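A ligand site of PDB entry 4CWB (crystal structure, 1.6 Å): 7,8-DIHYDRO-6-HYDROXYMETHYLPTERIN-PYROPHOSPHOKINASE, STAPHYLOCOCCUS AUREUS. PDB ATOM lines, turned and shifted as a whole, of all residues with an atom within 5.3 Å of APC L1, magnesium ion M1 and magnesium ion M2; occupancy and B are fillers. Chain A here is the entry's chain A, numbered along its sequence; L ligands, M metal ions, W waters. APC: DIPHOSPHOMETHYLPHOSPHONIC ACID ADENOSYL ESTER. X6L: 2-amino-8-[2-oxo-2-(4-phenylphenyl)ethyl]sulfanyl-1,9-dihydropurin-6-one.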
ATOM      1  N   LEU A  74     -17.014  18.251  -6.365  1.00  0.00           N
ATOM      2  CA  LEU A  74     -17.609  19.593  -6.370  1.00  0.00           C
ATOM      3  C   LEU A  74     -18.894  19.632  -7.210  1.00  0.00           C
ATOM      4  O   LEU A  74     -19.889  20.228  -6.800  1.00  0.00           O
ATOM      5  CB  LEU A  74     -16.634  20.638  -6.870  1.00  0.00           C
ATOM      6  CG  LEU A  74     -17.140  22.092  -6.847  1.00  0.00           C
ATOM      7  CD1 LEU A  74     -17.348  22.650  -5.438  1.00  0.00           C
ATOM      8  CD2 LEU A  74     -16.190  22.986  -7.608  1.00  0.00           C
ATOM      9  N   LEU A  78     -22.677  20.754  -5.931  1.00  0.00           N
ATOM     10  CA  LEU A  78     -23.507  21.763  -6.595  1.00  0.00           C
ATOM     11  C   LEU A  78     -24.808  21.191  -7.142  1.00  0.00           C
ATOM     12  O   LEU A  78     -25.848  21.855  -7.058  1.00  0.00           O
ATOM     13  CB  LEU A  78     -22.724  22.483  -7.708  1.00  0.00           C
ATOM     14  CG  LEU A  78     -21.468  23.204  -7.212  1.00  0.00           C
ATOM     15  CD1 LEU A  78     -20.740  23.903  -8.357  1.00  0.00           C
ATOM     16  CD2 LEU A  78     -21.769  24.180  -6.083  1.00  0.00           C
ATOM     17  N   GLU A  81     -27.308  20.873  -4.343  1.00  0.00           N
ATOM     18  CA  GLU A  81     -27.920  22.172  -4.080  1.00  0.00           C
ATOM     19  C   GLU A  81     -29.068  22.456  -5.054  1.00  0.00           C
ATOM     20  O   GLU A  81     -30.125  22.927  -4.649  1.00  0.00           O
ATOM     21  CB  GLU A  81     -26.873  23.280  -4.124  1.00  0.00           C
ATOM     22  CG  GLU A  81     -25.815  23.184  -3.022  1.00  0.00           C
ATOM     23  CD  GLU A  81     -24.778  24.275  -3.124  1.00  0.00           C
ATOM     24  OE1 GLU A  81     -24.845  25.102  -4.068  1.00  0.00           O
ATOM     25  OE2 GLU A  81     -23.863  24.337  -2.266  1.00  0.00           O
ATOM     26  N   ARG A  86     -31.911  25.353  -4.538  1.00  0.00           N
ATOM     27  CA  ARG A  86     -31.176  26.551  -4.239  1.00  0.00           C
ATOM     28  C   ARG A  86     -31.267  27.491  -5.434  1.00  0.00           C
ATOM     29  O   ARG A  86     -30.644  27.285  -6.472  1.00  0.00           O
ATOM     30  CB  ARG A  86     -29.700  26.264  -3.890  1.00  0.00           C
ATOM     31  CG  ARG A  86     -28.996  27.515  -3.423  1.00  0.00           C
ATOM     32  CD  ARG A  86     -27.522  27.313  -3.135  1.00  0.00           C
ATOM     33  NE  ARG A  86     -26.937  28.565  -2.648  1.00  0.00           N
ATOM     34  CZ  ARG A  86     -25.678  28.678  -2.224  1.00  0.00           C
ATOM     35  NH1 ARG A  86     -24.886  27.621  -2.224  1.00  0.00           N
ATOM     36  NH2 ARG A  86     -25.234  29.850  -1.819  1.00  0.00           N
ATOM     37  N   LYS A  89     -28.444  32.718  -5.249  1.00  0.00           N
ATOM     38  CA  LYS A  89     -27.016  32.524  -5.453  1.00  0.00           C
ATOM     39  C   LYS A  89     -26.138  33.638  -4.882  1.00  0.00           C
ATOM     40  O   LYS A  89     -24.905  33.582  -5.019  1.00  0.00           O
ATOM     41  CB  LYS A  89     -26.732  32.307  -6.952  1.00  0.00           C
ATOM     42  CG  LYS A  89     -27.371  31.043  -7.536  1.00  0.00           C
ATOM     43  CD  LYS A  89     -26.954  29.784  -6.779  1.00  0.00           C
ATOM     44  CE  LYS A  89     -27.691  28.545  -7.256  1.00  0.00           C
ATOM     45  NZ  LYS A  89     -26.874  27.757  -8.220  1.00  0.00           N
ATOM     46  N   GLU A  90     -26.736  34.635  -4.220  1.00  0.00           N
ATOM     47  CA  GLU A  90     -25.973  35.661  -3.494  1.00  0.00           C
ATOM     48  C   GLU A  90     -25.188  34.924  -2.453  1.00  0.00           C
ATOM     49  O   GLU A  90     -25.770  34.287  -1.563  1.00  0.00           O
ATOM     50  CB  GLU A  90     -26.874  36.690  -2.780  1.00  0.00           C
ATOM     51  CG  GLU A  90     -27.761  37.539  -3.680  1.00  0.00           C
ATOM     52  CD  GLU A  90     -28.951  36.784  -4.258  1.00  0.00           C
ATOM     53  OE1 GLU A  90     -29.387  35.755  -3.677  1.00  0.00           O
ATOM     54  OE2 GLU A  90     -29.457  37.220  -5.317  1.00  0.00           O
ATOM     55  N   ARG A  91     -23.864  34.998  -2.524  1.00  0.00           N
ATOM     56  CA  ARG A  91     -23.006  34.216  -1.656  1.00  0.00           C
ATOM     57  C   ARG A  91     -23.193  34.579  -0.209  1.00  0.00           C
ATOM     58  O   ARG A  91     -22.952  33.763   0.669  1.00  0.00           O
ATOM     59  CB  ARG A  91     -21.538  34.452  -2.005  1.00  0.00           C
ATOM     60  CG  ARG A  91     -21.079  33.889  -3.337  1.00  0.00           C
ATOM     61  CD  ARG A  91     -19.604  34.263  -3.518  1.00  0.00           C
ATOM     62  NE  ARG A  91     -18.769  33.787  -2.395  1.00  0.00           N
ATOM     63  CZ  ARG A  91     -17.856  32.825  -2.484  1.00  0.00           C
ATOM     64  NH1 ARG A  91     -17.624  32.197  -3.632  1.00  0.00           N
ATOM     65  NH2 ARG A  91     -17.160  32.471  -1.405  1.00  0.00           N
ATOM     66  N   ARG A  95     -30.004  30.416   1.809  1.00  0.00           N
ATOM     67  CA  ARG A  95     -30.018  29.297   0.886  1.00  0.00           C
ATOM     68  C   ARG A  95     -30.716  28.086   1.514  1.00  0.00           C
ATOM     69  O   ARG A  95     -30.582  27.809   2.700  1.00  0.00           O
ATOM     70  CB  ARG A  95     -28.604  28.906   0.384  1.00  0.00           C
ATOM     71  CG  ARG A  95     -27.668  28.212   1.381  1.00  0.00           C
ATOM     72  CD  ARG A  95     -27.145  29.088   2.511  1.00  0.00           C
ATOM     73  NE  ARG A  95     -26.537  30.320   2.027  1.00  0.00           N
ATOM     74  CZ  ARG A  95     -25.270  30.448   1.641  1.00  0.00           C
ATOM     75  NH1 ARG A  95     -24.408  29.439   1.772  1.00  0.00           N
ATOM     76  NH2 ARG A  95     -24.858  31.606   1.134  1.00  0.00           N
ATOM     77  N   ASP A  98     -26.497  24.463   1.263  1.00  0.00           N
ATOM     78  CA  ASP A  98     -25.107  24.715   0.913  1.00  0.00           C
ATOM     79  C   ASP A  98     -24.330  23.434   1.215  1.00  0.00           C
ATOM     80  O   ASP A  98     -24.446  22.885   2.309  1.00  0.00           O
ATOM     81  CB  ASP A  98     -24.567  25.856   1.776  1.00  0.00           C
ATOM     82  CG  ASP A  98     -23.140  26.224   1.444  1.00  0.00           C
ATOM     83  OD1 ASP A  98     -22.808  26.252   0.252  1.00  0.00           O
ATOM     84  OD2 ASP A  98     -22.382  26.556   2.400  1.00  0.00           O
ATOM     85  N   VAL A  99     -23.583  22.945   0.238  1.00  0.00           N
ATOM     86  CA  VAL A  99     -22.710  21.793   0.426  1.00  0.00           C
ATOM     87  C   VAL A  99     -21.284  22.244   0.058  1.00  0.00           C
ATOM     88  O   VAL A  99     -20.988  22.519  -1.114  1.00  0.00           O
ATOM     89  CB  VAL A  99     -23.105  20.598  -0.444  1.00  0.00           C
ATOM     90  CG1 VAL A  99     -22.266  19.390  -0.082  1.00  0.00           C
ATOM     91  CG2 VAL A  99     -24.583  20.257  -0.268  1.00  0.00           C
ATOM     92  N   ASP A 100     -20.405  22.269   1.054  1.00  0.00           N
ATOM     93  CA  ASP A 100     -19.044  22.759   0.895  1.00  0.00           C
ATOM     94  C   ASP A 100     -18.058  21.609   1.075  1.00  0.00           C
ATOM     95  O   ASP A 100     -18.251  20.764   1.958  1.00  0.00           O
ATOM     96  CB  ASP A 100     -18.729  23.841   1.925  1.00  0.00           C
ATOM     97  CG  ASP A 100     -19.495  25.121   1.692  1.00  0.00           C
ATOM     98  OD1 ASP A 100     -20.032  25.280   0.577  1.00  0.00           O
ATOM     99  OD2 ASP A 100     -19.572  25.934   2.629  1.00  0.00           O
ATOM    100  N   ILE A 101     -17.027  21.573   0.254  1.00  0.00           N
ATOM    101  CA  ILE A 101     -15.948  20.609   0.455  1.00  0.00           C
ATOM    102  C   ILE A 101     -14.999  21.180   1.504  1.00  0.00           C
ATOM    103  O   ILE A 101     -14.382  22.236   1.287  1.00  0.00           O
ATOM    104  CB  ILE A 101     -15.152  20.276  -0.830  1.00  0.00           C
ATOM    105  CG1 ILE A 101     -16.063  19.755  -1.931  1.00  0.00           C
ATOM    106  CG2 ILE A 101     -14.056  19.256  -0.494  1.00  0.00           C
ATOM    107  CD1 ILE A 101     -15.399  19.648  -3.313  1.00  0.00           C
ATOM    108  N   LEU A 102     -14.871  20.507   2.640  1.00  0.00           N
ATOM    109  CA  LEU A 102     -13.996  20.956   3.709  1.00  0.00           C
ATOM    110  C   LEU A 102     -12.581  20.393   3.582  1.00  0.00           C
ATOM    111  O   LEU A 102     -11.607  21.121   3.699  1.00  0.00           O
ATOM    112  CB  LEU A 102     -14.578  20.576   5.081  1.00  0.00           C
ATOM    113  CG  LEU A 102     -15.973  21.113   5.349  1.00  0.00           C
ATOM    114  CD1 LEU A 102     -16.487  20.615   6.699  1.00  0.00           C
ATOM    115  CD2 LEU A 102     -15.995  22.624   5.277  1.00  0.00           C
ATOM    116  N   LYS A 113     -11.456  29.412  -8.173  1.00  0.00           N
ATOM    117  CA  LYS A 113     -12.820  29.061  -7.772  1.00  0.00           C
ATOM    118  C   LYS A 113     -12.935  27.782  -6.942  1.00  0.00           C
ATOM    119  O   LYS A 113     -14.036  27.256  -6.761  1.00  0.00           O
ATOM    120  CB  LYS A 113     -13.697  28.934  -9.007  1.00  0.00           C
ATOM    121  CG  LYS A 113     -13.806  30.234  -9.801  1.00  0.00           C
ATOM    122  CD  LYS A 113     -14.768  30.074 -10.969  1.00  0.00           C
ATOM    123  CE  LYS A 113     -14.823  31.343 -11.819  1.00  0.00           C
ATOM    124  NZ  LYS A 113     -15.772  31.214 -12.962  1.00  0.00           N
ATOM    125  N   LEU A 114     -11.827  27.257  -6.448  1.00  0.00           N
ATOM    126  CA  LEU A 114     -11.901  26.067  -5.585  1.00  0.00           C
ATOM    127  C   LEU A 114     -10.702  25.989  -4.687  1.00  0.00           C
ATOM    128  O   LEU A 114      -9.560  25.859  -5.161  1.00  0.00           O
ATOM    129  CB  LEU A 114     -11.996  24.775  -6.397  1.00  0.00           C
ATOM    130  CG  LEU A 114     -11.945  23.478  -5.577  1.00  0.00           C
ATOM    131  CD1 LEU A 114     -13.160  23.331  -4.671  1.00  0.00           C
ATOM    132  CD2 LEU A 114     -11.870  22.294  -6.511  1.00  0.00           C
ATOM    133  N   SER A 115     -10.945  26.101  -3.376  1.00  0.00           N
ATOM    134  CA  SER A 115      -9.904  25.973  -2.382  1.00  0.00           C
ATOM    135  C   SER A 115     -10.307  24.842  -1.452  1.00  0.00           C
ATOM    136  O   SER A 115     -11.392  24.864  -0.847  1.00  0.00           O
ATOM    137  CB  SER A 115      -9.644  27.240  -1.565  1.00  0.00           C
ATOM    138  OG  SER A 115      -9.040  28.283  -2.342  1.00  0.00           O
ATOM    139  N   VAL A 116      -9.431  23.853  -1.349  1.00  0.00           N
ATOM    140  CA  VAL A 116      -9.600  22.739  -0.409  1.00  0.00           C
ATOM    141  C   VAL A 116      -8.227  22.539   0.226  1.00  0.00           C
ATOM    142  O   VAL A 116      -7.231  22.476  -0.497  1.00  0.00           O
ATOM    143  CB  VAL A 116      -9.995  21.438  -1.122  1.00  0.00           C
ATOM    144  CG1 VAL A 116     -10.074  20.256  -0.144  1.00  0.00           C
ATOM    145  CG2 VAL A 116     -11.310  21.608  -1.876  1.00  0.00           C
ATOM    146  N   HIS A 118     -11.196  23.916   2.778  1.00  0.00           N
ATOM    147  CA  HIS A 118     -11.982  25.123   2.689  1.00  0.00           C
ATOM    148  C   HIS A 118     -11.255  26.210   3.460  1.00  0.00           C
ATOM    149  O   HIS A 118     -10.912  26.028   4.617  1.00  0.00           O
ATOM    150  CB  HIS A 118     -13.370  24.883   3.268  1.00  0.00           C
ATOM    151  CG  HIS A 118     -14.331  25.965   2.895  1.00  0.00           C
ATOM    152  ND1 HIS A 118     -14.285  27.226   3.441  1.00  0.00           N
ATOM    153  CD2 HIS A 118     -15.321  25.978   1.967  1.00  0.00           C
ATOM    154  CE1 HIS A 118     -15.216  27.972   2.876  1.00  0.00           C
ATOM    155  NE2 HIS A 118     -15.865  27.250   1.988  1.00  0.00           N
ATOM    156  N   PRO A 119     -11.001  27.366   2.819  1.00  0.00           N
ATOM    157  CA  PRO A 119     -10.062  28.293   3.448  1.00  0.00           C
ATOM    158  C   PRO A 119     -10.619  29.104   4.601  1.00  0.00           C
ATOM    159  O   PRO A 119      -9.865  29.790   5.291  1.00  0.00           O
ATOM    160  CB  PRO A 119      -9.642  29.218   2.301  1.00  0.00           C
ATOM    161  CG  PRO A 119     -10.666  29.058   1.245  1.00  0.00           C
ATOM    162  CD  PRO A 119     -11.329  27.718   1.439  1.00  0.00           C
ATOM    163  N   ARG A 120     -11.941  29.009   4.851  1.00  0.00           N
ATOM    164  CA  ARG A 120     -12.562  29.718   5.939  1.00  0.00           C
ATOM    165  C   ARG A 120     -12.954  28.807   7.081  1.00  0.00           C
ATOM    166  O   ARG A 120     -13.435  29.275   8.106  1.00  0.00           O
ATOM    167  CB  ARG A 120     -13.762  30.508   5.409  1.00  0.00           C
ATOM    168  CG  ARG A 120     -13.321  31.725   4.597  1.00  0.00           C
ATOM    169  CD  ARG A 120     -14.392  32.231   3.663  1.00  0.00           C
ATOM    170  NE  ARG A 120     -14.476  31.499   2.412  1.00  0.00           N
ATOM    171  CZ  ARG A 120     -13.565  31.608   1.432  1.00  0.00           C
ATOM    172  NH1 ARG A 120     -12.501  32.393   1.586  1.00  0.00           N
ATOM    173  NH2 ARG A 120     -13.690  30.910   0.316  1.00  0.00           N
ATOM    174  N   ARG A 124     -14.517  29.223  11.672  1.00  0.00           N
ATOM    175  CA  ARG A 124     -15.980  29.059  11.751  1.00  0.00           C
ATOM    176  C   ARG A 124     -16.359  27.985  12.725  1.00  0.00           C
ATOM    177  O   ARG A 124     -16.167  26.795  12.454  1.00  0.00           O
ATOM    178  CB  ARG A 124     -16.568  28.731  10.401  1.00  0.00           C
ATOM    179  CG  ARG A 124     -16.425  29.829   9.371  1.00  0.00           C
ATOM    180  CD  ARG A 124     -16.762  29.326   7.995  1.00  0.00           C
ATOM    181  NE  ARG A 124     -16.912  30.420   7.036  1.00  0.00           N
ATOM    182  CZ  ARG A 124     -17.352  30.272   5.790  1.00  0.00           C
ATOM    183  NH1 ARG A 124     -17.697  29.072   5.302  1.00  0.00           N
ATOM    184  NH2 ARG A 124     -17.395  31.324   4.992  1.00  0.00           N
HETATM  185  PG  APC L   1     -18.346  29.544   1.758  1.00  0.00           P
HETATM  186  O1G APC L   1     -17.349  30.576   2.321  1.00  0.00           O
HETATM  187  O2G APC L   1     -17.785  28.725   0.609  1.00  0.00           O
HETATM  188  O3G APC L   1     -18.978  28.769   2.851  1.00  0.00           O
HETATM  189  PB  APC L   1     -20.773  29.847   0.348  1.00  0.00           P
HETATM  190  O1B APC L   1     -20.875  28.370   0.696  1.00  0.00           O
HETATM  191  O2B APC L   1     -22.048  30.701   0.791  1.00  0.00           O
HETATM  192  O3B APC L   1     -19.511  30.461   1.133  1.00  0.00           O
HETATM  193  PA  APC L   1     -21.418  29.245  -2.542  1.00  0.00           P
HETATM  194  O1A APC L   1     -21.940  27.965  -1.968  1.00  0.00           O
HETATM  195  O2A APC L   1     -22.563  30.314  -2.869  1.00  0.00           O
HETATM  196  C3A APC L   1     -20.318  30.039  -1.378  1.00  0.00           C
HETATM  197  O5' APC L   1     -20.542  28.714  -3.791  1.00  0.00           O
HETATM  198  C5' APC L   1     -19.910  29.549  -4.717  1.00  0.00           C
HETATM  199  C4' APC L   1     -18.631  28.875  -5.206  1.00  0.00           C
HETATM  200  O4' APC L   1     -17.697  28.709  -4.125  1.00  0.00           O
HETATM  201  C3' APC L   1     -18.714  27.483  -5.807  1.00  0.00           C
HETATM  202  O3' APC L   1     -19.344  27.401  -7.101  1.00  0.00           O
HETATM  203  C2' APC L   1     -17.226  27.167  -5.861  1.00  0.00           C
HETATM  204  O2' APC L   1     -16.648  27.581  -7.120  1.00  0.00           O
HETATM  205  C1' APC L   1     -16.638  28.012  -4.743  1.00  0.00           C
HETATM  206  N9  APC L   1     -15.834  27.199  -3.818  1.00  0.00           N
HETATM  207  C8  APC L   1     -14.521  27.405  -3.595  1.00  0.00           C
HETATM  208  N7  APC L   1     -14.013  26.497  -2.747  1.00  0.00           N
HETATM  209  C5  APC L   1     -15.051  25.657  -2.434  1.00  0.00           C
HETATM  210  C6  APC L   1     -15.196  24.474  -1.569  1.00  0.00           C
HETATM  211  N6  APC L   1     -14.145  23.992  -0.870  1.00  0.00           N
HETATM  212  N1  APC L   1     -16.424  23.934  -1.536  1.00  0.00           N
HETATM  213  C2  APC L   1     -17.483  24.394  -2.220  1.00  0.00           C
HETATM  214  N3  APC L   1     -17.415  25.478  -3.006  1.00  0.00           N
HETATM  215  C4  APC L   1     -16.239  26.117  -3.143  1.00  0.00           C
HETATM  216  C22 X6L L   2     -16.670  39.037   7.495  1.00  0.00           C
HETATM  217  C21 X6L L   2     -17.197  38.163   8.415  1.00  0.00           C
HETATM  218  C23 X6L L   2     -16.943  38.842   6.171  1.00  0.00           C
HETATM  219  C20 X6L L   2     -17.975  37.110   7.995  1.00  0.00           C
HETATM  220  C24 X6L L   2     -17.730  37.786   5.756  1.00  0.00           C
HETATM  221  C15 X6L L   2     -19.802  35.845   5.019  1.00  0.00           C
HETATM  222  C17 X6L L   2     -18.948  34.518   6.781  1.00  0.00           C
HETATM  223  C14 X6L L   2     -20.439  34.737   4.510  1.00  0.00           C
HETATM  224  C18 X6L L   2     -19.572  33.405   6.271  1.00  0.00           C
HETATM  225  C19 X6L L   2     -18.267  36.903   6.671  1.00  0.00           C
HETATM  226  C16 X6L L   2     -19.035  35.770   6.165  1.00  0.00           C
HETATM  227  C13 X6L L   2     -20.318  33.515   5.123  1.00  0.00           C
HETATM  228  C5  X6L L   2     -23.701  30.265   6.944  1.00  0.00           C
HETATM  229  C4  X6L L   2     -23.734  31.359   7.728  1.00  0.00           C
HETATM  230  C7  X6L L   2     -23.622  31.901   5.616  1.00  0.00           C
HETATM  231  C25 X6L L   2     -23.756  28.973   7.575  1.00  0.00           C
HETATM  232  C2  X6L L   2     -23.899  30.299   9.624  1.00  0.00           C
HETATM  233  C11 X6L L   2     -20.959  32.307   4.555  1.00  0.00           C
HETATM  234  C10 X6L L   2     -22.047  32.373   3.538  1.00  0.00           C
HETATM  235  N6  X6L L   2     -23.620  30.592   5.610  1.00  0.00           N
HETATM  236  N3  X6L L   2     -23.827  31.464   9.050  1.00  0.00           N
HETATM  237  N8  X6L L   2     -23.659  32.432   6.875  1.00  0.00           N
HETATM  238  N27 X6L L   2     -23.868  29.102   8.948  1.00  0.00           N
HETATM  239  N1  X6L L   2     -24.016  30.159  10.953  1.00  0.00           N
HETATM  240  O26 X6L L   2     -23.748  27.904   6.998  1.00  0.00           O
HETATM  241  O12 X6L L   2     -20.575  31.221   4.897  1.00  0.00           O
HETATM  242  S9  X6L L   2     -23.570  32.969   4.235  1.00  0.00           S
HETATM  243 MG    MG M   1     -20.599  27.626   2.559  1.00  0.00          MG
HETATM  244 MG    MG M   2     -21.046  26.703  -0.601  1.00  0.00          MG
HETATM  245  O   HOH W   1     -21.563  28.941   3.742  1.00  0.00           O
HETATM  246  O   HOH W   2     -20.125  33.468   0.892  1.00  0.00           O
HETATM  247  O   HOH W   3     -22.044  27.639  -7.110  1.00  0.00           O
HETATM  248  O   HOH W   4     -23.439  30.987  -5.146  1.00  0.00           O
HETATM  249  O   HOH W   5     -15.919  29.701  -0.975  1.00  0.00           O
HETATM  250  O   HOH W   6     -20.919  26.926   5.131  1.00  0.00           O
HETATM  251  O   HOH W   7     -17.456  33.045   1.317  1.00  0.00           O
HETATM  252  O   HOH W   8     -21.294  25.178  -1.949  1.00  0.00           O
HETATM  253  O   HOH W   9     -19.107  27.196  -1.278  1.00  0.00           O
HETATM  254  O   HOH W  10     -12.862  30.235  -4.197  1.00  0.00           O
HETATM  255  O   HOH W  11     -15.148  31.105  -5.252  1.00  0.00           O
HETATM  256  O   HOH W  12     -22.802  26.661  -4.589  1.00  0.00           O
HETATM  257  O   HOH W  13     -18.795  32.435  -6.264  1.00  0.00           O
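The guanidinium group of Arg 95 sits close to the side-chain carboxylate of Asp 98 (3.6 Å).
The side-chain carboxylate (OD1) of Asp 98 lies close to the guanidinium group (NH1) of Arg 86 (3.5 Å).
The backbone NH (N) of Arg 120 sits close to a ring nitrogen (ND1) of His 118 (3.3 Å).
N of His 118 sits at hydrogen-bond distance from O of Leu 102 (3.0 Å).
The guanidinium group of Arg 95 is in hydrogen-bond range of the backbone carbonyl oxygen of Arg 91, at 2.9 Å.
NH1 of Arg 86 lies within salt-bridge range of OE1 of Glu 81, 3.1 Å away.
The backbone carbonyl oxygen (O) of Lys 113 lies within hydrogen-bond range of an oxygen (O2') of APC L1 (2.7 Å).
An oxygen (O1G) of APC L1 is in salt-bridge range of the guanidinium group (NH2) of Arg 124 (2.8 Å).
An oxygen (O2G) of APC L1 sits at hydrogen-bond distance from a ring nitrogen (NE2) of His 118 (2.8 Å).
The backbone NH (N) of Ile 101 lies within hydrogen-bond range of a nitrogen (N1) of APC L1 (3.0 Å).
The backbone carbonyl oxygen (O) of Ile 101 is in hydrogen-bond range of a nitrogen (N6) of APC L1 (2.8 Å).
An oxygen (O2B) of APC L1 is in salt-bridge range of the guanidinium group (NH1) of Arg 95, at 2.9 Å.
N of Ser 115 is in hydrogen-bond range of N7 of APC L1, at 3.2 Å.
A nitrogen (N6) of APC L1 lies within hydrogen-bond range of the backbone carbonyl oxygen (O) of Ser 115 (2.9 Å).
NH2 of Arg 86 is in salt-bridge range of O2A of APC L1.
NE of Arg 120 is in salt-bridge range of O1G of APC L1 (3.0 Å).
The guanidinium group (NH2) of Arg 124 sits at hydrogen-bond distance from an oxygen (O12) of X6L L2.
The guanidinium group (NH2) of Arg 95 lies close to a sulfur (S9) of X6L L2 (3.6 Å).
Water W1 lies within hydrogen-bond range of O12 of X6L L2 (2.7 Å), O2B of APC L1 (3.5 Å) and NH1 of Arg 95 (3.5 Å).
Water W8 lies within hydrogen-bond range of OE2 of Glu 81 (2.7 Å) and O of Val 99 (2.8 Å).
Water W5 lies within hydrogen-bond range of an oxygen (O2G) of APC L1, the guanidinium group of Arg 120 and the guanidinium group of Arg 91.
Water W7 bridges O1G of APC L1 and NH2 of Arg 91.
Water W12 lies within hydrogen-bond range of the side-chain carboxylate of Glu 81 (2.6 Å), an oxygen (O5') of APC L1 (3.2 Å) and the guanidinium group of Arg 86 (3.3 Å).
Water W2 bridges the backbone carbonyl oxygen (O) of Arg 91 (2.9 Å) and an oxygen (O3B) of APC L1 (3.1 Å).
Magnesium ion M2 is bound by the side-chain carboxylate of Asp 98 (2.0 Å), water W8 (2.1 Å), an oxygen (O1A) of APC L1 (2.1 Å), the side-chain carboxylate of Asp 100 (2.1 Å), water W9 (2.1 Å) and an oxygen (O1B) of APC L1 (2.1 Å).
Magnesium ion M2 has six donor atoms within binding distance.
Two residues have an atom within 4 Å of magnesium ion M2: Asp 98 and Asp 100.
The nearest printed residue that does not touch magnesium ion M2 is Glu 81 (4.04 Å).
Magnesium ion M1 is bound by the side-chain carboxylate of Asp 100 (2.0 Å), an oxygen (O3G) of APC L1 (2.0 Å), water W1 (2.0 Å), an oxygen (O1B) of APC L1 (2.0 Å) and the side-chain carboxylate of Asp 98 (2.1 Å).
Slightly farther from magnesium ion M1 lies water W6 (2.7 Å).
O of Arg 91 lies close to O2B of APC L1 (3.2 Å).
Residues that only touch APC L1: Leu 114, Leu 74, Val 116 and Leu 78.
Hydrophobic or aromatic side chains within 4 Å of APC L1: Leu 74, Leu 78, Ile 101, Leu 114, Val 116 and His 118.
15 residues have an atom within 4 Å of APC L1: Leu 74, Leu 78, Arg 86, Arg 91, Arg 95, Asp 98, Asp 100, Ile 101, Lys 113, Leu 114, Ser 115, Val 116, His 118, Arg 120 and Arg 124.
Two residues have an atom within 4 Å of magnesium ion M1: Asp 98 and Asp 100.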
